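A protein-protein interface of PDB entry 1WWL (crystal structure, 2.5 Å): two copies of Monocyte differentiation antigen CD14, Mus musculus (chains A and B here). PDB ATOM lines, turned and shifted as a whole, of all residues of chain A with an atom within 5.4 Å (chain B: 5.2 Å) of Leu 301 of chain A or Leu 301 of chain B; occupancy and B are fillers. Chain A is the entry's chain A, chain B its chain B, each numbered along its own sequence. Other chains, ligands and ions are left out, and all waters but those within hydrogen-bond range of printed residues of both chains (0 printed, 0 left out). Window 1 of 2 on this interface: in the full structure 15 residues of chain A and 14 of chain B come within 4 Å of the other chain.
Among the printed residues, pairs that only touch across the chains: Ser 302 of chain A with Gly 299 of chain B (3.3 Å), Gly 299 of chain A with Ser 302 of chain B (3.3 Å), Gly 299 of chain A with Leu 301 of chain B (3.7 Å), Leu 303 of chain A with Val 298 of chain B (3.8 Å), Leu 301 of chain A with Gly 299 of chain B (3.8 Å) and Val 298 of chain A with Leu 303 of chain B (3.9 Å).
Of the 9 printed residues of chain A, 6 touch a printed residue of chain B. Among the printed residues, no Asp or Glu carboxylate lies within 4 Å of a Lys or Arg side-chain nitrogen of the other chain.
O of Asn 300 of chain A is in hydrogen-bond range of N of Leu 279 of chain A (3.0 Å). The backbone carbonyl oxygen of Leu 279 of chain A sits at hydrogen-bond distance from the backbone NH of Ser 302 of chain A (3.3 Å). N of Leu 281 of chain A sits at hydrogen-bond distance from O of Ser 302 of chain A, 2.8 Å away. O of Asn 300 of chain B is in hydrogen-bond range of N of Leu 279 of chain B, at 3.0 Å. The backbone NH (N) of Ser 302 of chain B lies within hydrogen-bond range of the backbone carbonyl oxygen (O) of Leu 279 of chain B. O of Ser 302 of chain B is in hydrogen-bond range of N of Leu 281 of chain B (3.0 Å).
O of Gly 299 of chain A lies within hydrogen-bond range of N of Leu 303 of chain B, 2.7 Å away. ND2 of Asn 300 of chain B lies close to ND2 of Asn 300 of chain A, 3.3 Å away. The side-chain amide nitrogen (ND2) of Asn 300 of chain A lies close to the backbone carbonyl oxygen (O) of Leu 301 of chain B, at 3.4 Å. ND2 of Asn 300 of chain B lies within hydrogen-bond range of O of Leu 301 of chain A, 3.2 Å away. O of Leu 301 of chain A lies within hydrogen-bond range of N of Leu 301 of chain B, 2.7 Å away. The backbone NH (N) of Leu 303 of chain A sits at hydrogen-bond distance from the backbone carbonyl oxygen (O) of Gly 299 of chain B (2.6 Å).
Leu 301 of chain A touches just these residues of chain B: Gly 299 (3.8 Å), Asn 300 (3.2 Å) and Leu 301 (2.7 Å). Of the printed residues of chain B, Ser 302 of chain A touches Gly 299. Leu 301 of chain B touches just these residues of chain A: Gly 299, Asn 300 and Leu 301. Of the printed residues of chain A, Leu 303 of chain B touches Val 298 (3.9 Å) and Gly 299 (2.7 Å). The nearest residue of chain B that does not touch Leu 301 of chain A is Ser 302 of chain B (5.0 Å).
Gly 299 of chain A touches Ser 302 of chain B, and with the chains exchanged Ser 302 of chain A touches Gly 299 of chain B. Gly 299 of chain A touches Leu 303 of chain B, and with the chains exchanged Leu 303 of chain A touches Gly 299 of chain B. Asn 300 of chain A touches Leu 301 of chain B, and with the chains exchanged Leu 301 of chain A touches Asn 300 of chain B. Leu 301 of chain B touches its own counterpart, Leu 301 of chain A. Positions printed for both chains: 279, 281, 295, 298, 299, 300, 301, 302 and 303. Of the 12 pairs that touch across the chains among the printed residues, 12 have their exchanged pair printed and touching as well.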
ATOM      1  N   LEU A 279     -29.823  13.982  16.244  1.00  0.00           N
ATOM      2  CA  LEU A 279     -28.676  13.357  16.864  1.00  0.00           C
ATOM      3  C   LEU A 279     -28.452  14.121  18.169  1.00  0.00           C
ATOM      4  O   LEU A 279     -27.990  15.255  18.141  1.00  0.00           O
ATOM      5  CB  LEU A 279     -27.427  13.490  15.977  1.00  0.00           C
ATOM      6  CG  LEU A 279     -26.177  12.613  16.251  1.00  0.00           C
ATOM      7  CD1 LEU A 279     -24.904  13.296  15.749  1.00  0.00           C
ATOM      8  CD2 LEU A 279     -25.997  12.353  17.715  1.00  0.00           C
ATOM      9  N   LEU A 281     -26.278  14.703  21.174  1.00  0.00           N
ATOM     10  CA  LEU A 281     -24.924  14.444  21.664  1.00  0.00           C
ATOM     11  C   LEU A 281     -24.616  15.250  22.944  1.00  0.00           C
ATOM     12  O   LEU A 281     -23.450  15.450  23.332  1.00  0.00           O
ATOM     13  CB  LEU A 281     -23.952  14.802  20.529  1.00  0.00           C
ATOM     14  CG  LEU A 281     -22.851  13.857  20.004  1.00  0.00           C
ATOM     15  CD1 LEU A 281     -23.118  12.427  20.394  1.00  0.00           C
ATOM     16  CD2 LEU A 281     -22.710  14.011  18.487  1.00  0.00           C
ATOM     17  N   LEU A 295     -19.114  14.669  11.735  1.00  0.00           N
ATOM     18  CA  LEU A 295     -20.535  14.553  12.044  1.00  0.00           C
ATOM     19  C   LEU A 295     -21.390  14.181  10.849  1.00  0.00           C
ATOM     20  O   LEU A 295     -21.000  14.414   9.706  1.00  0.00           O
ATOM     21  CB  LEU A 295     -21.007  15.903  12.591  1.00  0.00           C
ATOM     22  CG  LEU A 295     -21.678  16.158  13.946  1.00  0.00           C
ATOM     23  CD1 LEU A 295     -21.372  15.090  14.984  1.00  0.00           C
ATOM     24  CD2 LEU A 295     -21.220  17.530  14.405  1.00  0.00           C
ATOM     25  N   VAL A 298     -27.323  16.353  10.001  1.00  0.00           N
ATOM     26  CA  VAL A 298     -28.352  16.302  11.032  1.00  0.00           C
ATOM     27  C   VAL A 298     -29.360  17.435  10.916  1.00  0.00           C
ATOM     28  O   VAL A 298     -28.965  18.582  10.749  1.00  0.00           O
ATOM     29  CB  VAL A 298     -27.679  16.379  12.456  1.00  0.00           C
ATOM     30  CG1 VAL A 298     -28.716  16.430  13.525  1.00  0.00           C
ATOM     31  CG2 VAL A 298     -26.768  15.184  12.685  1.00  0.00           C
ATOM     32  N   GLY A 299     -30.651  17.116  11.010  1.00  0.00           N
ATOM     33  CA  GLY A 299     -31.662  18.156  10.976  1.00  0.00           C
ATOM     34  C   GLY A 299     -31.752  18.817  12.357  1.00  0.00           C
ATOM     35  O   GLY A 299     -31.971  20.022  12.501  1.00  0.00           O
ATOM     36  N   ASN A 300     -31.549  18.030  13.401  1.00  0.00           N
ATOM     37  CA  ASN A 300     -31.626  18.563  14.736  1.00  0.00           C
ATOM     38  C   ASN A 300     -30.452  18.044  15.557  1.00  0.00           C
ATOM     39  O   ASN A 300     -30.420  16.885  15.944  1.00  0.00           O
ATOM     40  CB  ASN A 300     -32.952  18.140  15.340  1.00  0.00           C
ATOM     41  CG  ASN A 300     -33.415  19.072  16.423  1.00  0.00           C
ATOM     42  OD1 ASN A 300     -34.623  19.227  16.632  1.00  0.00           O
ATOM     43  ND2 ASN A 300     -32.465  19.696  17.136  1.00  0.00           N
ATOM     44  N   LEU A 301     -29.491  18.918  15.817  1.00  0.00           N
ATOM     45  CA  LEU A 301     -28.301  18.548  16.542  1.00  0.00           C
ATOM     46  C   LEU A 301     -28.172  19.234  17.880  1.00  0.00           C
ATOM     47  O   LEU A 301     -28.270  20.452  17.997  1.00  0.00           O
ATOM     48  CB  LEU A 301     -27.071  18.856  15.706  1.00  0.00           C
ATOM     49  CG  LEU A 301     -25.710  18.570  16.341  1.00  0.00           C
ATOM     50  CD1 LEU A 301     -25.508  17.053  16.535  1.00  0.00           C
ATOM     51  CD2 LEU A 301     -24.622  19.156  15.432  1.00  0.00           C
ATOM     52  N   SER A 302     -27.909  18.429  18.893  1.00  0.00           N
ATOM     53  CA  SER A 302     -27.770  18.929  20.245  1.00  0.00           C
ATOM     54  C   SER A 302     -26.362  18.610  20.782  1.00  0.00           C
ATOM     55  O   SER A 302     -25.891  17.478  20.702  1.00  0.00           O
ATOM     56  CB  SER A 302     -28.868  18.299  21.106  1.00  0.00           C
ATOM     57  OG  SER A 302     -29.320  19.196  22.105  1.00  0.00           O
ATOM     58  N   LEU A 303     -25.686  19.630  21.300  1.00  0.00           N
ATOM     59  CA  LEU A 303     -24.345  19.480  21.850  1.00  0.00           C
ATOM     60  C   LEU A 303     -24.267  20.193  23.195  1.00  0.00           C
ATOM     61  O   LEU A 303     -23.190  20.315  23.792  1.00  0.00           O
ATOM     62  CB  LEU A 303     -23.310  20.070  20.889  1.00  0.00           C
ATOM     63  CG  LEU A 303     -23.041  19.273  19.597  1.00  0.00           C
ATOM     64  CD1 LEU A 303     -22.277  20.154  18.609  1.00  0.00           C
ATOM     65  CD2 LEU A 303     -22.244  17.985  19.907  1.00  0.00           C
ATOM     66  N   LEU B 279     -29.378  28.046  17.753  1.00  0.00           N
ATOM     67  CA  LEU B 279     -29.363  28.635  16.451  1.00  0.00           C
ATOM     68  C   LEU B 279     -30.352  27.823  15.647  1.00  0.00           C
ATOM     69  O   LEU B 279     -30.076  26.678  15.275  1.00  0.00           O
ATOM     70  CB  LEU B 279     -27.977  28.520  15.812  1.00  0.00           C
ATOM     71  CG  LEU B 279     -27.544  29.567  14.750  1.00  0.00           C
ATOM     72  CD1 LEU B 279     -27.277  28.897  13.440  1.00  0.00           C
ATOM     73  CD2 LEU B 279     -28.590  30.665  14.569  1.00  0.00           C
ATOM     74  N   LEU B 281     -31.948  27.491  12.278  1.00  0.00           N
ATOM     75  CA  LEU B 281     -31.799  27.814  10.863  1.00  0.00           C
ATOM     76  C   LEU B 281     -32.707  26.941   9.987  1.00  0.00           C
ATOM     77  O   LEU B 281     -32.425  26.752   8.803  1.00  0.00           O
ATOM     78  CB  LEU B 281     -30.367  27.524  10.462  1.00  0.00           C
ATOM     79  CG  LEU B 281     -29.414  28.495   9.794  1.00  0.00           C
ATOM     80  CD1 LEU B 281     -29.891  29.936   9.848  1.00  0.00           C
ATOM     81  CD2 LEU B 281     -28.074  28.281  10.496  1.00  0.00           C
ATOM     82  N   LEU B 295     -20.426  27.761  10.480  1.00  0.00           N
ATOM     83  CA  LEU B 295     -21.382  27.885  11.578  1.00  0.00           C
ATOM     84  C   LEU B 295     -20.683  28.260  12.881  1.00  0.00           C
ATOM     85  O   LEU B 295     -19.457  28.161  12.994  1.00  0.00           O
ATOM     86  CB  LEU B 295     -22.075  26.543  11.767  1.00  0.00           C
ATOM     87  CG  LEU B 295     -23.550  26.263  11.513  1.00  0.00           C
ATOM     88  CD1 LEU B 295     -24.218  27.332  10.721  1.00  0.00           C
ATOM     89  CD2 LEU B 295     -23.640  24.939  10.820  1.00  0.00           C
ATOM     90  N   VAL B 298     -22.547  25.837  18.507  1.00  0.00           N
ATOM     91  CA  VAL B 298     -23.950  25.850  18.916  1.00  0.00           C
ATOM     92  C   VAL B 298     -24.326  24.689  19.841  1.00  0.00           C
ATOM     93  O   VAL B 298     -23.881  23.577  19.642  1.00  0.00           O
ATOM     94  CB  VAL B 298     -24.818  25.867  17.613  1.00  0.00           C
ATOM     95  CG1 VAL B 298     -26.303  25.703  17.895  1.00  0.00           C
ATOM     96  CG2 VAL B 298     -24.540  27.180  16.874  1.00  0.00           C
ATOM     97  N   GLY B 299     -25.122  24.976  20.867  1.00  0.00           N
ATOM     98  CA  GLY B 299     -25.565  23.937  21.762  1.00  0.00           C
ATOM     99  C   GLY B 299     -26.705  23.181  21.088  1.00  0.00           C
ATOM    100  O   GLY B 299     -26.757  21.943  21.128  1.00  0.00           O
ATOM    101  N   ASN B 300     -27.618  23.925  20.461  1.00  0.00           N
ATOM    102  CA  ASN B 300     -28.767  23.324  19.787  1.00  0.00           C
ATOM    103  C   ASN B 300     -28.949  23.897  18.379  1.00  0.00           C
ATOM    104  O   ASN B 300     -29.265  25.074  18.215  1.00  0.00           O
ATOM    105  CB  ASN B 300     -30.038  23.558  20.598  1.00  0.00           C
ATOM    106  CG  ASN B 300     -31.157  22.612  20.212  1.00  0.00           C
ATOM    107  OD1 ASN B 300     -32.236  22.626  20.817  1.00  0.00           O
ATOM    108  ND2 ASN B 300     -30.912  21.781  19.203  1.00  0.00           N
ATOM    109  N   LEU B 301     -28.757  23.049  17.377  1.00  0.00           N
ATOM    110  CA  LEU B 301     -28.852  23.475  16.011  1.00  0.00           C
ATOM    111  C   LEU B 301     -29.967  22.763  15.287  1.00  0.00           C
ATOM    112  O   LEU B 301     -30.144  21.531  15.377  1.00  0.00           O
ATOM    113  CB  LEU B 301     -27.539  23.215  15.305  1.00  0.00           C
ATOM    114  CG  LEU B 301     -27.401  23.768  13.887  1.00  0.00           C
ATOM    115  CD1 LEU B 301     -27.513  25.316  13.877  1.00  0.00           C
ATOM    116  CD2 LEU B 301     -26.036  23.308  13.346  1.00  0.00           C
ATOM    117  N   SER B 302     -30.726  23.567  14.556  1.00  0.00           N
ATOM    118  CA  SER B 302     -31.843  23.060  13.805  1.00  0.00           C
ATOM    119  C   SER B 302     -31.636  23.441  12.348  1.00  0.00           C
ATOM    120  O   SER B 302     -31.295  24.577  12.022  1.00  0.00           O
ATOM    121  CB  SER B 302     -33.141  23.620  14.370  1.00  0.00           C
ATOM    122  OG  SER B 302     -34.220  22.799  13.976  1.00  0.00           O
ATOM    123  N   LEU B 303     -31.815  22.462  11.475  1.00  0.00           N
ATOM    124  CA  LEU B 303     -31.607  22.657  10.049  1.00  0.00           C
ATOM    125  C   LEU B 303     -32.672  21.900   9.294  1.00  0.00           C
ATOM    126  O   LEU B 303     -32.635  21.794   8.076  1.00  0.00           O
ATOM    127  CB  LEU B 303     -30.245  22.117   9.646  1.00  0.00           C
ATOM    128  CG  LEU B 303     -29.009  22.967   9.909  1.00  0.00           C
ATOM    129  CD1 LEU B 303     -27.779  22.196   9.435  1.00  0.00           C
ATOM    130  CD2 LEU B 303     -29.103  24.270   9.175  1.00  0.00           C
